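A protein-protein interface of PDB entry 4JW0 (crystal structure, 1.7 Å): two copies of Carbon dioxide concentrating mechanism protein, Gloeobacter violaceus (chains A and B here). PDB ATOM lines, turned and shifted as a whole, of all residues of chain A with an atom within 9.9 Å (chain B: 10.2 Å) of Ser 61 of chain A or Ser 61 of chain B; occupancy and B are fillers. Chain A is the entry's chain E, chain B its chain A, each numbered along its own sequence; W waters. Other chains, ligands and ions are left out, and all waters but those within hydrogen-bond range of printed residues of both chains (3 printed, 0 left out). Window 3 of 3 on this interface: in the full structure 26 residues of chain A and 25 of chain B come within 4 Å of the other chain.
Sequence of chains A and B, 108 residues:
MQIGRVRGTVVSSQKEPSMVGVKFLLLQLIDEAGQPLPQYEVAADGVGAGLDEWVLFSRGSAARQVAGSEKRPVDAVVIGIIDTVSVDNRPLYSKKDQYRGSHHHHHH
Water W3 lies within hydrogen-bond range of NH1 of Arg 64 of chain B (2.5 Å), O of Val 74 of chain B (2.8 Å), N of Ala 62 of chain A (3.4 Å) and O of Gly 60 of chain B (3.5 Å). Water W1 bridges NH2 of Arg 64 of chain B (2.7 Å) and OG of Ser 61 of chain A (3.5 Å). Water W2 lies within hydrogen-bond range of O of Lys 71 of chain B (2.8 Å) and O of Gln 65 of chain A (3.2 Å).
OG of Ser 61 of chain A is in hydrogen-bond range of NH1 of Arg 64 of chain B. OG of Ser 58 of chain A is in hydrogen-bond range of O of Pro 73 of chain B (2.8 Å). The backbone NH (N) of Arg 59 of chain A is in hydrogen-bond range of the side-chain carboxylate (OD2) of Asp 75 of chain B, 2.8 Å away.
Ser 61 of chain A touches just these residues of chain B: Ser 61 and Arg 64. Of chain B, only Arg 64 (3.5 Å), Pro 73 (3.3 Å) and Val 74 (3.8 Å) come within 4 Å of Ala 62 of chain A. Ala 63 of chain A touches none of the printed residues of chain B. No residue of chain B comes within 4 Å of Arg 64 of chain A. Of the printed residues of chain B, Ile 79 of chain A touches Pro 73 (3.5 Å). Arg 59 of chain B touches none of the printed residues of chain A. Ser 61 of chain B touches just one residue of chain A: Ser 61 (3.7 Å). No residue of chain A comes within 4 Å of Ala 62 of chain B. No residue of chain A comes within 4 Å of Ala 63 of chain B. Of the printed residues of chain A, Arg 64 of chain B touches Ser 61 (2.8 Å), Ala 62 (3.5 Å) and Gln 65 (3.5 Å). Of the printed residues of chain A, Glu 70 of chain B touches Gln 65 (3.7 Å). Of the printed residues of chain A, Asp 75 of chain B touches Ser 58 (3.3 Å) and Arg 59 (2.8 Å). Ala 76 of chain B touches none of the printed residues of chain A. The nearest residue of chain B that does not touch Ser 61 of chain A is Gly 60 of chain B (5.5 Å).
CB of Ser 61 of chain B touches OG of Ser 61 of chain A, 3.7 Å away. Ala 62 of chain A touches Arg 64 of chain B (N to NH1, 3.5 Å). Pro 73 of chain B touches Ala 62 of chain A (CB to O, 3.3 Å). Ala 62 of chain A touches Val 74 of chain B. CZ of Arg 64 of chain B touches NE2 of Gln 65 of chain A, at 3.5 Å. Gln 65 of chain A touches Glu 70 of chain B. O of Lys 71 of chain B touches CB of Gln 65 of chain A (3.6 Å). Gln 65 of chain A touches Arg 72 of chain B. N of Pro 73 of chain B touches CB of Gln 65 of chain A (3.8 Å). Ile 79 of chain A touches Pro 73 of chain B (CG2 to O, 3.5 Å).
Of the 20 printed residues of chain A, 6 touch a printed residue of chain B. Hydrophobic or aromatic side chains of chain A within 4 Å of the printed part of chain B: Ala 62 and Ile 79. Among the printed residues, 14 pairs touch across the chains.
The backbone carbonyl oxygen of Asp 75 of chain B is in hydrogen-bond range of the backbone NH of Gly 60 of chain B (2.8 Å). O of Ser 61 of chain B lies within hydrogen-bond range of NE2 of Gln 65 of chain B (3.1 Å). The backbone NH (N) of Glu 70 of chain B sits close to the backbone carbonyl oxygen (O) of Arg 64 of chain B, at 3.4 Å. The guanidinium group of Arg 72 of chain B is in hydrogen-bond range of the side-chain hydroxyl of Ser 69 of chain B. N of Ser 58 of chain A lies within hydrogen-bond range of O of Val 77 of chain A. O of Ser 61 of chain A is in hydrogen-bond range of NE2 of Gln 65 of chain A (3.0 Å).
Ser 61 of chain A touches Arg 64 of chain B, but with the chains exchanged Arg 64 of chain A does not touch Ser 61 of chain B (7.7 Å). Gln 65 of chain A touches Glu 70 of chain B, but with the chains exchanged Glu 70 of chain A does not touch Gln 65 of chain B (13.9 Å). Gln 65 of chain A touches Pro 73 of chain B, but with the chains exchanged Pro 73 of chain A does not touch Gln 65 of chain B (18.4 Å). Positions printed for both chains: 58, 59, 60, 61, 62, 63, 64, 65, 66, 67, 69, 70, 71, 72, 73, 74, 75, 76, 77 and 79.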
ATOM      1  N   SER A  58      24.972 -29.020 -12.897  1.00  0.00           N
ATOM      2  CA  SER A  58      24.566 -27.916 -13.757  1.00  0.00           C
ATOM      3  C   SER A  58      24.715 -28.323 -15.198  1.00  0.00           C
ATOM      4  O   SER A  58      25.551 -29.156 -15.523  1.00  0.00           O
ATOM      5  CB  SER A  58      25.433 -26.689 -13.496  1.00  0.00           C
ATOM      6  OG  SER A  58      25.162 -26.160 -12.219  1.00  0.00           O
ATOM      7  N   ARG A  59      23.902 -27.716 -16.053  1.00  0.00           N
ATOM      8  CA  ARG A  59      23.911 -27.993 -17.479  1.00  0.00           C
ATOM      9  C   ARG A  59      24.266 -26.749 -18.266  1.00  0.00           C
ATOM     10  O   ARG A  59      24.055 -25.629 -17.806  1.00  0.00           O
ATOM     11  CB  ARG A  59      22.533 -28.468 -17.927  1.00  0.00           C
ATOM     12  CG  ARG A  59      22.149 -29.828 -17.400  1.00  0.00           C
ATOM     13  CD  ARG A  59      20.680 -30.089 -17.639  1.00  0.00           C
ATOM     14  NE  ARG A  59      20.381 -31.514 -17.549  1.00  0.00           N
ATOM     15  CZ  ARG A  59      19.252 -32.020 -17.067  1.00  0.00           C
ATOM     16  NH1 ARG A  59      18.287 -31.226 -16.623  1.00  0.00           N
ATOM     17  NH2 ARG A  59      19.090 -33.334 -17.027  1.00  0.00           N
ATOM     18  N   GLY A  60      24.782 -26.954 -19.470  1.00  0.00           N
ATOM     19  CA  GLY A  60      25.089 -25.855 -20.360  1.00  0.00           C
ATOM     20  C   GLY A  60      26.475 -25.296 -20.116  1.00  0.00           C
ATOM     21  O   GLY A  60      27.365 -25.999 -19.632  1.00  0.00           O
ATOM     22  N   SER A  61      26.655 -24.022 -20.452  1.00  0.00           N
ATOM     23  CA  SER A  61      27.963 -23.379 -20.379  1.00  0.00           C
ATOM     24  C   SER A  61      28.471 -23.255 -18.946  1.00  0.00           C
ATOM     25  O   SER A  61      29.652 -22.996 -18.725  1.00  0.00           O
ATOM     26  CB  SER A  61      27.943 -22.009 -21.079  1.00  0.00           C
ATOM     27  OG  SER A  61      26.941 -21.163 -20.552  1.00  0.00           O
ATOM     28  N   ALA A  62      27.577 -23.449 -17.981  1.00  0.00           N
ATOM     29  CA  ALA A  62      27.964 -23.548 -16.581  1.00  0.00           C
ATOM     30  C   ALA A  62      29.085 -24.572 -16.419  1.00  0.00           C
ATOM     31  O   ALA A  62      29.958 -24.430 -15.560  1.00  0.00           O
ATOM     32  CB  ALA A  62      26.771 -23.962 -15.747  1.00  0.00           C
ATOM     33  N   ALA A  63      29.051 -25.616 -17.239  1.00  0.00           N
ATOM     34  CA  ALA A  63      30.006 -26.711 -17.105  1.00  0.00           C
ATOM     35  C   ALA A  63      31.428 -26.287 -17.446  1.00  0.00           C
ATOM     36  O   ALA A  63      32.383 -26.944 -17.040  1.00  0.00           O
ATOM     37  CB  ALA A  63      29.588 -27.882 -17.978  1.00  0.00           C
ATOM     38  N   ARG A  64      31.567 -25.202 -18.200  1.00  0.00           N
ATOM     39  CA  ARG A  64      32.882 -24.732 -18.625  1.00  0.00           C
ATOM     40  C   ARG A  64      33.519 -23.755 -17.629  1.00  0.00           C
ATOM     41  O   ARG A  64      34.626 -23.276 -17.854  1.00  0.00           O
ATOM     42  CB  ARG A  64      32.794 -24.068 -20.006  1.00  0.00           C
ATOM     43  CG  ARG A  64      32.213 -24.953 -21.098  1.00  0.00           C
ATOM     44  CD  ARG A  64      32.538 -24.429 -22.495  1.00  0.00           C
ATOM     45  NE  ARG A  64      32.218 -23.013 -22.689  1.00  0.00           N
ATOM     46  CZ  ARG A  64      31.067 -22.552 -23.172  1.00  0.00           C
ATOM     47  NH1 ARG A  64      30.092 -23.375 -23.510  1.00  0.00           N
ATOM     48  NH2 ARG A  64      30.887 -21.251 -23.318  1.00  0.00           N
ATOM     49  N   GLN A  65      32.838 -23.460 -16.528  1.00  0.00           N
ATOM     50  CA  GLN A  65      33.296 -22.390 -15.639  1.00  0.00           C
ATOM     51  C   GLN A  65      34.378 -22.840 -14.662  1.00  0.00           C
ATOM     52  O   GLN A  65      35.139 -22.014 -14.157  1.00  0.00           O
ATOM     53  CB  GLN A  65      32.119 -21.791 -14.869  1.00  0.00           C
ATOM     54  CG  GLN A  65      31.074 -21.175 -15.764  1.00  0.00           C
ATOM     55  CD  GLN A  65      31.673 -20.299 -16.834  1.00  0.00           C
ATOM     56  OE1 GLN A  65      32.441 -19.385 -16.544  1.00  0.00           O
ATOM     57  NE2 GLN A  65      31.334 -20.577 -18.087  1.00  0.00           N
ATOM     58  N   VAL A  66      34.452 -24.141 -14.400  1.00  0.00           N
ATOM     59  CA  VAL A  66      35.468 -24.675 -13.494  1.00  0.00           C
ATOM     60  C   VAL A  66      36.853 -24.562 -14.126  1.00  0.00           C
ATOM     61  O   VAL A  66      37.037 -24.877 -15.298  1.00  0.00           O
ATOM     62  CB  VAL A  66      35.183 -26.147 -13.108  1.00  0.00           C
ATOM     63  CG1 VAL A  66      33.825 -26.268 -12.437  1.00  0.00           C
ATOM     64  CG2 VAL A  66      35.250 -27.054 -14.326  1.00  0.00           C
ATOM     65  N   ALA A  67      37.825 -24.097 -13.349  1.00  0.00           N
ATOM     66  CA  ALA A  67      39.190 -23.960 -13.845  1.00  0.00           C
ATOM     67  C   ALA A  67      39.612 -25.213 -14.605  1.00  0.00           C
ATOM     68  O   ALA A  67      39.496 -26.326 -14.098  1.00  0.00           O
ATOM     69  CB  ALA A  67      40.148 -23.685 -12.695  1.00  0.00           C
ATOM     70  N   SER A  69      38.266 -26.092 -17.606  1.00  0.00           N
ATOM     71  CA  SER A  69      37.212 -26.509 -18.533  1.00  0.00           C
ATOM     72  C   SER A  69      36.691 -25.384 -19.417  1.00  0.00           C
ATOM     73  O   SER A  69      35.737 -25.573 -20.164  1.00  0.00           O
ATOM     74  CB  SER A  69      36.048 -27.111 -17.752  1.00  0.00           C
ATOM     75  OG  SER A  69      36.448 -28.316 -17.133  1.00  0.00           O
ATOM     76  N   GLU A  70      37.323 -24.221 -19.340  1.00  0.00           N
ATOM     77  CA  GLU A  70      36.820 -23.040 -20.026  1.00  0.00           C
ATOM     78  C   GLU A  70      36.616 -23.267 -21.529  1.00  0.00           C
ATOM     79  O   GLU A  70      35.686 -22.710 -22.122  1.00  0.00           O
ATOM     80  CB  GLU A  70      37.751 -21.853 -19.779  1.00  0.00           C
ATOM     81  CG  GLU A  70      37.750 -21.368 -18.323  1.00  0.00           C
ATOM     82  CD  GLU A  70      38.820 -22.021 -17.459  1.00  0.00           C
ATOM     83  OE1 GLU A  70      39.460 -23.005 -17.901  1.00  0.00           O
ATOM     84  OE2 GLU A  70      39.023 -21.538 -16.325  1.00  0.00           O
ATOM     85  N   LYS A  71      37.471 -24.082 -22.136  1.00  0.00           N
ATOM     86  CA  LYS A  71      37.383 -24.344 -23.571  1.00  0.00           C
ATOM     87  C   LYS A  71      37.137 -25.829 -23.872  1.00  0.00           C
ATOM     88  O   LYS A  71      37.487 -26.323 -24.945  1.00  0.00           O
ATOM     89  CB  LYS A  71      38.649 -23.848 -24.282  1.00  0.00           C
ATOM     90  CG  LYS A  71      38.720 -22.325 -24.441  1.00  0.00           C
ATOM     91  CD  LYS A  71      40.161 -21.822 -24.377  1.00  0.00           C
ATOM     92  CE  LYS A  71      40.329 -20.432 -24.995  1.00  0.00           C
ATOM     93  NZ  LYS A  71      39.490 -19.381 -24.349  1.00  0.00           N
ATOM     94  N   ARG A  72      36.514 -26.533 -22.931  1.00  0.00           N
ATOM     95  CA  ARG A  72      36.123 -27.921 -23.153  1.00  0.00           C
ATOM     96  C   ARG A  72      34.680 -28.017 -23.637  1.00  0.00           C
ATOM     97  O   ARG A  72      33.831 -27.229 -23.216  1.00  0.00           O
ATOM     98  CB  ARG A  72      36.251 -28.732 -21.872  1.00  0.00           C
ATOM     99  CG  ARG A  72      37.679 -28.984 -21.433  1.00  0.00           C
ATOM    100  CD  ARG A  72      37.695 -29.854 -20.197  1.00  0.00           C
ATOM    101  NE  ARG A  72      39.044 -30.320 -19.889  1.00  0.00           N
ATOM    102  CZ  ARG A  72      39.550 -30.420 -18.665  1.00  0.00           C
ATOM    103  NH1 ARG A  72      38.834 -30.088 -17.598  1.00  0.00           N
ATOM    104  NH2 ARG A  72      40.789 -30.859 -18.508  1.00  0.00           N
ATOM    105  N   PRO A  73      34.398 -28.997 -24.509  1.00  0.00           N
ATOM    106  CA  PRO A  73      33.048 -29.218 -25.042  1.00  0.00           C
ATOM    107  C   PRO A  73      32.177 -30.006 -24.076  1.00  0.00           C
ATOM    108  O   PRO A  73      31.603 -31.030 -24.450  1.00  0.00           O
ATOM    109  CB  PRO A  73      33.308 -30.019 -26.315  1.00  0.00           C
ATOM    110  CG  PRO A  73      34.535 -30.776 -26.013  1.00  0.00           C
ATOM    111  CD  PRO A  73      35.390 -29.846 -25.190  1.00  0.00           C
ATOM    112  N   VAL A  74      32.086 -29.516 -22.842  1.00  0.00           N
ATOM    113  CA  VAL A  74      31.284 -30.149 -21.793  1.00  0.00           C
ATOM    114  C   VAL A  74      30.040 -29.324 -21.484  1.00  0.00           C
ATOM    115  O   VAL A  74      30.100 -28.093 -21.418  1.00  0.00           O
ATOM    116  CB  VAL A  74      32.094 -30.349 -20.481  1.00  0.00           C
ATOM    117  CG1 VAL A  74      33.116 -31.452 -20.654  1.00  0.00           C
ATOM    118  CG2 VAL A  74      32.764 -29.053 -20.042  1.00  0.00           C
ATOM    119  N   ASP A  75      28.916 -30.012 -21.282  1.00  0.00           N
ATOM    120  CA  ASP A  75      27.634 -29.357 -21.049  1.00  0.00           C
ATOM    121  C   ASP A  75      26.930 -29.863 -19.782  1.00  0.00           C
ATOM    122  O   ASP A  75      25.748 -29.587 -19.560  1.00  0.00           O
ATOM    123  CB  ASP A  75      26.712 -29.552 -22.258  1.00  0.00           C
ATOM    124  CG  ASP A  75      26.255 -30.988 -22.422  1.00  0.00           C
ATOM    125  OD1 ASP A  75      26.805 -31.869 -21.729  1.00  0.00           O
ATOM    126  OD2 ASP A  75      25.348 -31.242 -23.252  1.00  0.00           O
ATOM    127  N   ALA A  76      27.651 -30.592 -18.942  1.00  0.00           N
ATOM    128  CA  ALA A  76      27.112 -30.998 -17.651  1.00  0.00           C
ATOM    129  C   ALA A  76      28.273 -31.193 -16.679  1.00  0.00           C
ATOM    130  O   ALA A  76      29.299 -31.776 -17.030  1.00  0.00           O
ATOM    131  CB  ALA A  76      26.305 -32.270 -17.780  1.00  0.00           C
ATOM    132  N   VAL A  77      28.098 -30.692 -15.464  1.00  0.00           N
ATOM    133  CA  VAL A  77      29.154 -30.724 -14.460  1.00  0.00           C
ATOM    134  C   VAL A  77      28.583 -30.971 -13.069  1.00  0.00           C
ATOM    135  O   VAL A  77      27.532 -30.424 -12.702  1.00  0.00           O
ATOM    136  CB  VAL A  77      29.959 -29.400 -14.460  1.00  0.00           C
ATOM    137  CG1 VAL A  77      29.067 -28.219 -14.095  1.00  0.00           C
ATOM    138  CG2 VAL A  77      31.144 -29.487 -13.509  1.00  0.00           C
ATOM    139  N   ILE A  79      28.741 -30.142  -9.379  1.00  0.00           N
ATOM    140  CA  ILE A  79      29.259 -29.000  -8.634  1.00  0.00           C
ATOM    141  C   ILE A  79      29.381 -29.268  -7.134  1.00  0.00           C
ATOM    142  O   ILE A  79      30.038 -28.509  -6.426  1.00  0.00           O
ATOM    143  CB  ILE A  79      28.434 -27.718  -8.885  1.00  0.00           C
ATOM    144  CG1 ILE A  79      27.011 -27.863  -8.347  1.00  0.00           C
ATOM    145  CG2 ILE A  79      28.418 -27.398 -10.363  1.00  0.00           C
ATOM    146  CD1 ILE A  79      26.216 -26.580  -8.403  1.00  0.00           C
ATOM    147  N   SER B  58      15.490 -17.841 -13.496  1.00  0.00           N
ATOM    148  CA  SER B  58      16.041 -18.015 -14.832  1.00  0.00           C
ATOM    149  C   SER B  58      16.987 -19.210 -14.875  1.00  0.00           C
ATOM    150  O   SER B  58      17.584 -19.587 -13.863  1.00  0.00           O
ATOM    151  CB  SER B  58      16.794 -16.757 -15.265  1.00  0.00           C
ATOM    152  OG  SER B  58      15.910 -15.659 -15.357  1.00  0.00           O
ATOM    153  N   ARG B  59      17.124 -19.788 -16.063  1.00  0.00           N
ATOM    154  CA  ARG B  59      18.005 -20.921 -16.283  1.00  0.00           C
ATOM    155  C   ARG B  59      19.101 -20.578 -17.291  1.00  0.00           C
ATOM    156  O   ARG B  59      18.943 -19.690 -18.138  1.00  0.00           O
ATOM    157  CB  ARG B  59      17.209 -22.111 -16.813  1.00  0.00           C
ATOM    158  CG  ARG B  59      16.140 -22.652 -15.881  1.00  0.00           C
ATOM    159  CD  ARG B  59      15.426 -23.798 -16.564  1.00  0.00           C
ATOM    160  NE  ARG B  59      14.373 -24.411 -15.761  1.00  0.00           N
ATOM    161  CZ  ARG B  59      13.072 -24.173 -15.906  1.00  0.00           C
ATOM    162  NH1 ARG B  59      12.630 -23.317 -16.819  1.00  0.00           N
ATOM    163  NH2 ARG B  59      12.201 -24.800 -15.130  1.00  0.00           N
ATOM    164  N   GLY B  60      20.206 -21.303 -17.205  1.00  0.00           N
ATOM    165  CA  GLY B  60      21.295 -21.152 -18.152  1.00  0.00           C
ATOM    166  C   GLY B  60      22.287 -20.093 -17.728  1.00  0.00           C
ATOM    167  O   GLY B  60      22.413 -19.779 -16.546  1.00  0.00           O
ATOM    168  N   SER B  61      22.985 -19.529 -18.707  1.00  0.00           N
ATOM    169  CA  SER B  61      24.042 -18.562 -18.439  1.00  0.00           C
ATOM    170  C   SER B  61      23.515 -17.275 -17.803  1.00  0.00           C
ATOM    171  O   SER B  61      24.293 -16.467 -17.304  1.00  0.00           O
ATOM    172  CB  SER B  61      24.793 -18.238 -19.731  1.00  0.00           C
ATOM    173  OG  SER B  61      23.902 -17.758 -20.718  1.00  0.00           O
ATOM    174  N   ALA B  62      22.196 -17.095 -17.831  1.00  0.00           N
ATOM    175  CA  ALA B  62      21.546 -16.014 -17.099  1.00  0.00           C
ATOM    176  C   ALA B  62      21.991 -16.006 -15.638  1.00  0.00           C
ATOM    177  O   ALA B  62      22.132 -14.950 -15.029  1.00  0.00           O
ATOM    178  CB  ALA B  62      20.043 -16.169 -17.174  1.00  0.00           C
ATOM    179  N   ALA B  63      22.215 -17.191 -15.081  1.00  0.00           N
ATOM    180  CA  ALA B  63      22.540 -17.309 -13.665  1.00  0.00           C
ATOM    181  C   ALA B  63      23.904 -16.709 -13.352  1.00  0.00           C
ATOM    182  O   ALA B  63      24.178 -16.351 -12.204  1.00  0.00           O
ATOM    183  CB  ALA B  63      22.486 -18.768 -13.228  1.00  0.00           C
ATOM    184  N   ARG B  64      24.748 -16.587 -14.373  1.00  0.00           N
ATOM    185  CA  ARG B  64      26.097 -16.055 -14.188  1.00  0.00           C
ATOM    186  C   ARG B  64      26.164 -14.531 -14.338  1.00  0.00           C
ATOM    187  O   ARG B  64      27.241 -13.944 -14.254  1.00  0.00           O
ATOM    188  CB  ARG B  64      27.075 -16.710 -15.168  1.00  0.00           C
ATOM    189  CG  ARG B  64      27.180 -18.224 -15.033  1.00  0.00           C
ATOM    190  CD  ARG B  64      28.459 -18.757 -15.650  1.00  0.00           C
ATOM    191  NE  ARG B  64      28.712 -18.249 -17.005  1.00  0.00           N
ATOM    192  CZ  ARG B  64      28.271 -18.822 -18.119  1.00  0.00           C
ATOM    193  NH1 ARG B  64      27.535 -19.920 -18.066  1.00  0.00           N
ATOM    194  NH2 ARG B  64      28.560 -18.293 -19.297  1.00  0.00           N
ATOM    195  N   GLN B  65      25.022 -13.889 -14.553  1.00  0.00           N
ATOM    196  CA  GLN B  65      25.014 -12.451 -14.796  1.00  0.00           C
ATOM    197  C   GLN B  65      24.993 -11.650 -13.498  1.00  0.00           C
ATOM    198  O   GLN B  65      25.310 -10.455 -13.493  1.00  0.00           O
ATOM    199  CB  GLN B  65      23.827 -12.060 -15.679  1.00  0.00           C
ATOM    200  CG  GLN B  65      23.827 -12.751 -17.041  1.00  0.00           C
ATOM    201  CD  GLN B  65      25.185 -12.693 -17.723  1.00  0.00           C
ATOM    202  OE1 GLN B  65      25.756 -11.618 -17.908  1.00  0.00           O
ATOM    203  NE2 GLN B  65      25.717 -13.855 -18.087  1.00  0.00           N
ATOM    204  N   VAL B  66      24.639 -12.310 -12.399  1.00  0.00           N
ATOM    205  CA  VAL B  66      24.599 -11.657 -11.095  1.00  0.00           C
ATOM    206  C   VAL B  66      26.017 -11.447 -10.580  1.00  0.00           C
ATOM    207  O   VAL B  66      26.842 -12.362 -10.623  1.00  0.00           O
ATOM    208  CB  VAL B  66      23.806 -12.500 -10.086  1.00  0.00           C
ATOM    209  CG1 VAL B  66      23.790 -11.832  -8.724  1.00  0.00           C
ATOM    210  CG2 VAL B  66      22.385 -12.726 -10.593  1.00  0.00           C
ATOM    211  N   ALA B  67      26.299 -10.240 -10.100  1.00  0.00           N
ATOM    212  CA  ALA B  67      27.628  -9.914  -9.594  1.00  0.00           C
ATOM    213  C   ALA B  67      28.120 -10.999  -8.640  1.00  0.00           C
ATOM    214  O   ALA B  67      27.411 -11.400  -7.709  1.00  0.00           O
ATOM    215  CB  ALA B  67      27.614  -8.570  -8.904  1.00  0.00           C
ATOM    216  N   SER B  69      28.959 -14.067  -9.668  1.00  0.00           N
ATOM    217  CA  SER B  69      28.698 -15.388 -10.234  1.00  0.00           C
ATOM    218  C   SER B  69      29.143 -15.541 -11.682  1.00  0.00           C
ATOM    219  O   SER B  69      28.844 -16.550 -12.318  1.00  0.00           O
ATOM    220  CB  SER B  69      27.210 -15.719 -10.112  1.00  0.00           C
ATOM    221  OG  SER B  69      26.860 -15.853  -8.749  1.00  0.00           O
ATOM    222  N   GLU B  70      29.875 -14.554 -12.187  1.00  0.00           N
ATOM    223  CA  GLU B  70      30.323 -14.550 -13.576  1.00  0.00           C
ATOM    224  C   GLU B  70      31.084 -15.813 -13.979  1.00  0.00           C
ATOM    225  O   GLU B  70      30.975 -16.273 -15.116  1.00  0.00           O
ATOM    226  CB  GLU B  70      31.197 -13.321 -13.841  1.00  0.00           C
ATOM    227  CG  GLU B  70      30.427 -12.003 -13.840  1.00  0.00           C
ATOM    228  CD  GLU B  70      30.342 -11.353 -12.467  1.00  0.00           C
ATOM    229  OE1 GLU B  70      30.758 -11.981 -11.466  1.00  0.00           O
ATOM    230  OE2 GLU B  70      29.857 -10.203 -12.394  1.00  0.00           O
ATOM    231  N   LYS B  71      31.852 -16.373 -13.053  1.00  0.00           N
ATOM    232  CA  LYS B  71      32.629 -17.572 -13.346  1.00  0.00           C
ATOM    233  C   LYS B  71      32.257 -18.746 -12.439  1.00  0.00           C
ATOM    234  O   LYS B  71      33.075 -19.632 -12.201  1.00  0.00           O
ATOM    235  CB  LYS B  71      34.127 -17.279 -13.233  1.00  0.00           C
ATOM    236  CG  LYS B  71      34.677 -16.399 -14.343  1.00  0.00           C
ATOM    237  CD  LYS B  71      36.121 -16.021 -14.055  1.00  0.00           C
ATOM    238  CE  LYS B  71      36.836 -15.476 -15.283  1.00  0.00           C
ATOM    239  NZ  LYS B  71      38.281 -15.233 -14.999  1.00  0.00           N
ATOM    240  N   ARG B  72      31.023 -18.760 -11.945  1.00  0.00           N
ATOM    241  CA  ARG B  72      30.525 -19.897 -11.184  1.00  0.00           C
ATOM    242  C   ARG B  72      29.768 -20.861 -12.096  1.00  0.00           C
ATOM    243  O   ARG B  72      29.077 -20.425 -13.015  1.00  0.00           O
ATOM    244  CB  ARG B  72      29.587 -19.435 -10.079  1.00  0.00           C
ATOM    245  CG  ARG B  72      30.278 -18.744  -8.921  1.00  0.00           C
ATOM    246  CD  ARG B  72      29.290 -18.421  -7.826  1.00  0.00           C
ATOM    247  NE  ARG B  72      29.974 -17.988  -6.607  1.00  0.00           N
ATOM    248  CZ  ARG B  72      29.503 -17.083  -5.757  1.00  0.00           C
ATOM    249  NH1 ARG B  72      28.335 -16.496  -5.970  1.00  0.00           N
ATOM    250  NH2 ARG B  72      30.209 -16.766  -4.680  1.00  0.00           N
ATOM    251  N   PRO B  73      29.886 -22.174 -11.833  1.00  0.00           N
ATOM    252  CA  PRO B  73      29.182 -23.209 -12.604  1.00  0.00           C
ATOM    253  C   PRO B  73      27.723 -23.331 -12.166  1.00  0.00           C
ATOM    254  O   PRO B  73      27.257 -24.399 -11.768  1.00  0.00           O
ATOM    255  CB  PRO B  73      29.969 -24.481 -12.283  1.00  0.00           C
ATOM    256  CG  PRO B  73      30.551 -24.224 -10.927  1.00  0.00           C
ATOM    257  CD  PRO B  73      30.840 -22.757 -10.869  1.00  0.00           C
ATOM    258  N   VAL B  74      27.012 -22.214 -12.252  1.00  0.00           N
ATOM    259  CA  VAL B  74      25.635 -22.125 -11.793  1.00  0.00           C
ATOM    260  C   VAL B  74      24.732 -21.925 -13.010  1.00  0.00           C
ATOM    261  O   VAL B  74      25.071 -21.161 -13.912  1.00  0.00           O
ATOM    262  CB  VAL B  74      25.491 -20.970 -10.763  1.00  0.00           C
ATOM    263  CG1 VAL B  74      25.780 -19.614 -11.411  1.00  0.00           C
ATOM    264  CG2 VAL B  74      24.135 -20.988 -10.111  1.00  0.00           C
ATOM    265  N   ASP B  75      23.612 -22.646 -13.054  1.00  0.00           N
ATOM    266  CA  ASP B  75      22.719 -22.638 -14.219  1.00  0.00           C
ATOM    267  C   ASP B  75      21.264 -22.320 -13.865  1.00  0.00           C
ATOM    268  O   ASP B  75      20.366 -22.503 -14.687  1.00  0.00           O
ATOM    269  CB  ASP B  75      22.776 -23.979 -14.954  1.00  0.00           C
ATOM    270  CG  ASP B  75      22.132 -25.110 -14.168  1.00  0.00           C
ATOM    271  OD1 ASP B  75      21.849 -24.924 -12.964  1.00  0.00           O
ATOM    272  OD2 ASP B  75      21.903 -26.189 -14.759  1.00  0.00           O
ATOM    273  N   ALA B  76      21.028 -21.862 -12.642  1.00  0.00           N
ATOM    274  CA  ALA B  76      19.693 -21.432 -12.240  1.00  0.00           C
ATOM    275  C   ALA B  76      19.807 -20.393 -11.136  1.00  0.00           C
ATOM    276  O   ALA B  76      20.619 -20.534 -10.223  1.00  0.00           O
ATOM    277  CB  ALA B  76      18.851 -22.632 -11.783  1.00  0.00           C
ATOM    278  N   VAL B  77      19.004 -19.340 -11.238  1.00  0.00           N
ATOM    279  CA  VAL B  77      19.080 -18.230 -10.303  1.00  0.00           C
ATOM    280  C   VAL B  77      17.704 -17.648  -9.996  1.00  0.00           C
ATOM    281  O   VAL B  77      16.873 -17.475 -10.887  1.00  0.00           O
ATOM    282  CB  VAL B  77      19.990 -17.106 -10.858  1.00  0.00           C
ATOM    283  CG1 VAL B  77      19.456 -16.590 -12.192  1.00  0.00           C
ATOM    284  CG2 VAL B  77      20.118 -15.969  -9.860  1.00  0.00           C
ATOM    285  N   ILE B  79      15.680 -14.514  -9.477  1.00  0.00           N
ATOM    286  CA  ILE B  79      15.888 -13.120  -9.860  1.00  0.00           C
ATOM    287  C   ILE B  79      14.954 -12.168  -9.117  1.00  0.00           C
ATOM    288  O   ILE B  79      15.209 -10.967  -9.050  1.00  0.00           O
ATOM    289  CB  ILE B  79      15.794 -12.895 -11.394  1.00  0.00           C
ATOM    290  CG1 ILE B  79      14.404 -13.240 -11.935  1.00  0.00           C
ATOM    291  CG2 ILE B  79      16.858 -13.712 -12.106  1.00  0.00           C
ATOM    292  CD1 ILE B  79      14.200 -12.808 -13.386  1.00  0.00           C
HETATM  293  O   HOH W   1      28.196 -18.250 -22.009  1.00  0.00           O
HETATM  294  O   HOH W   2      35.599 -20.467 -11.376  1.00  0.00           O
HETATM  295  O   HOH W   3      25.690 -20.884 -16.657  1.00  0.00           O
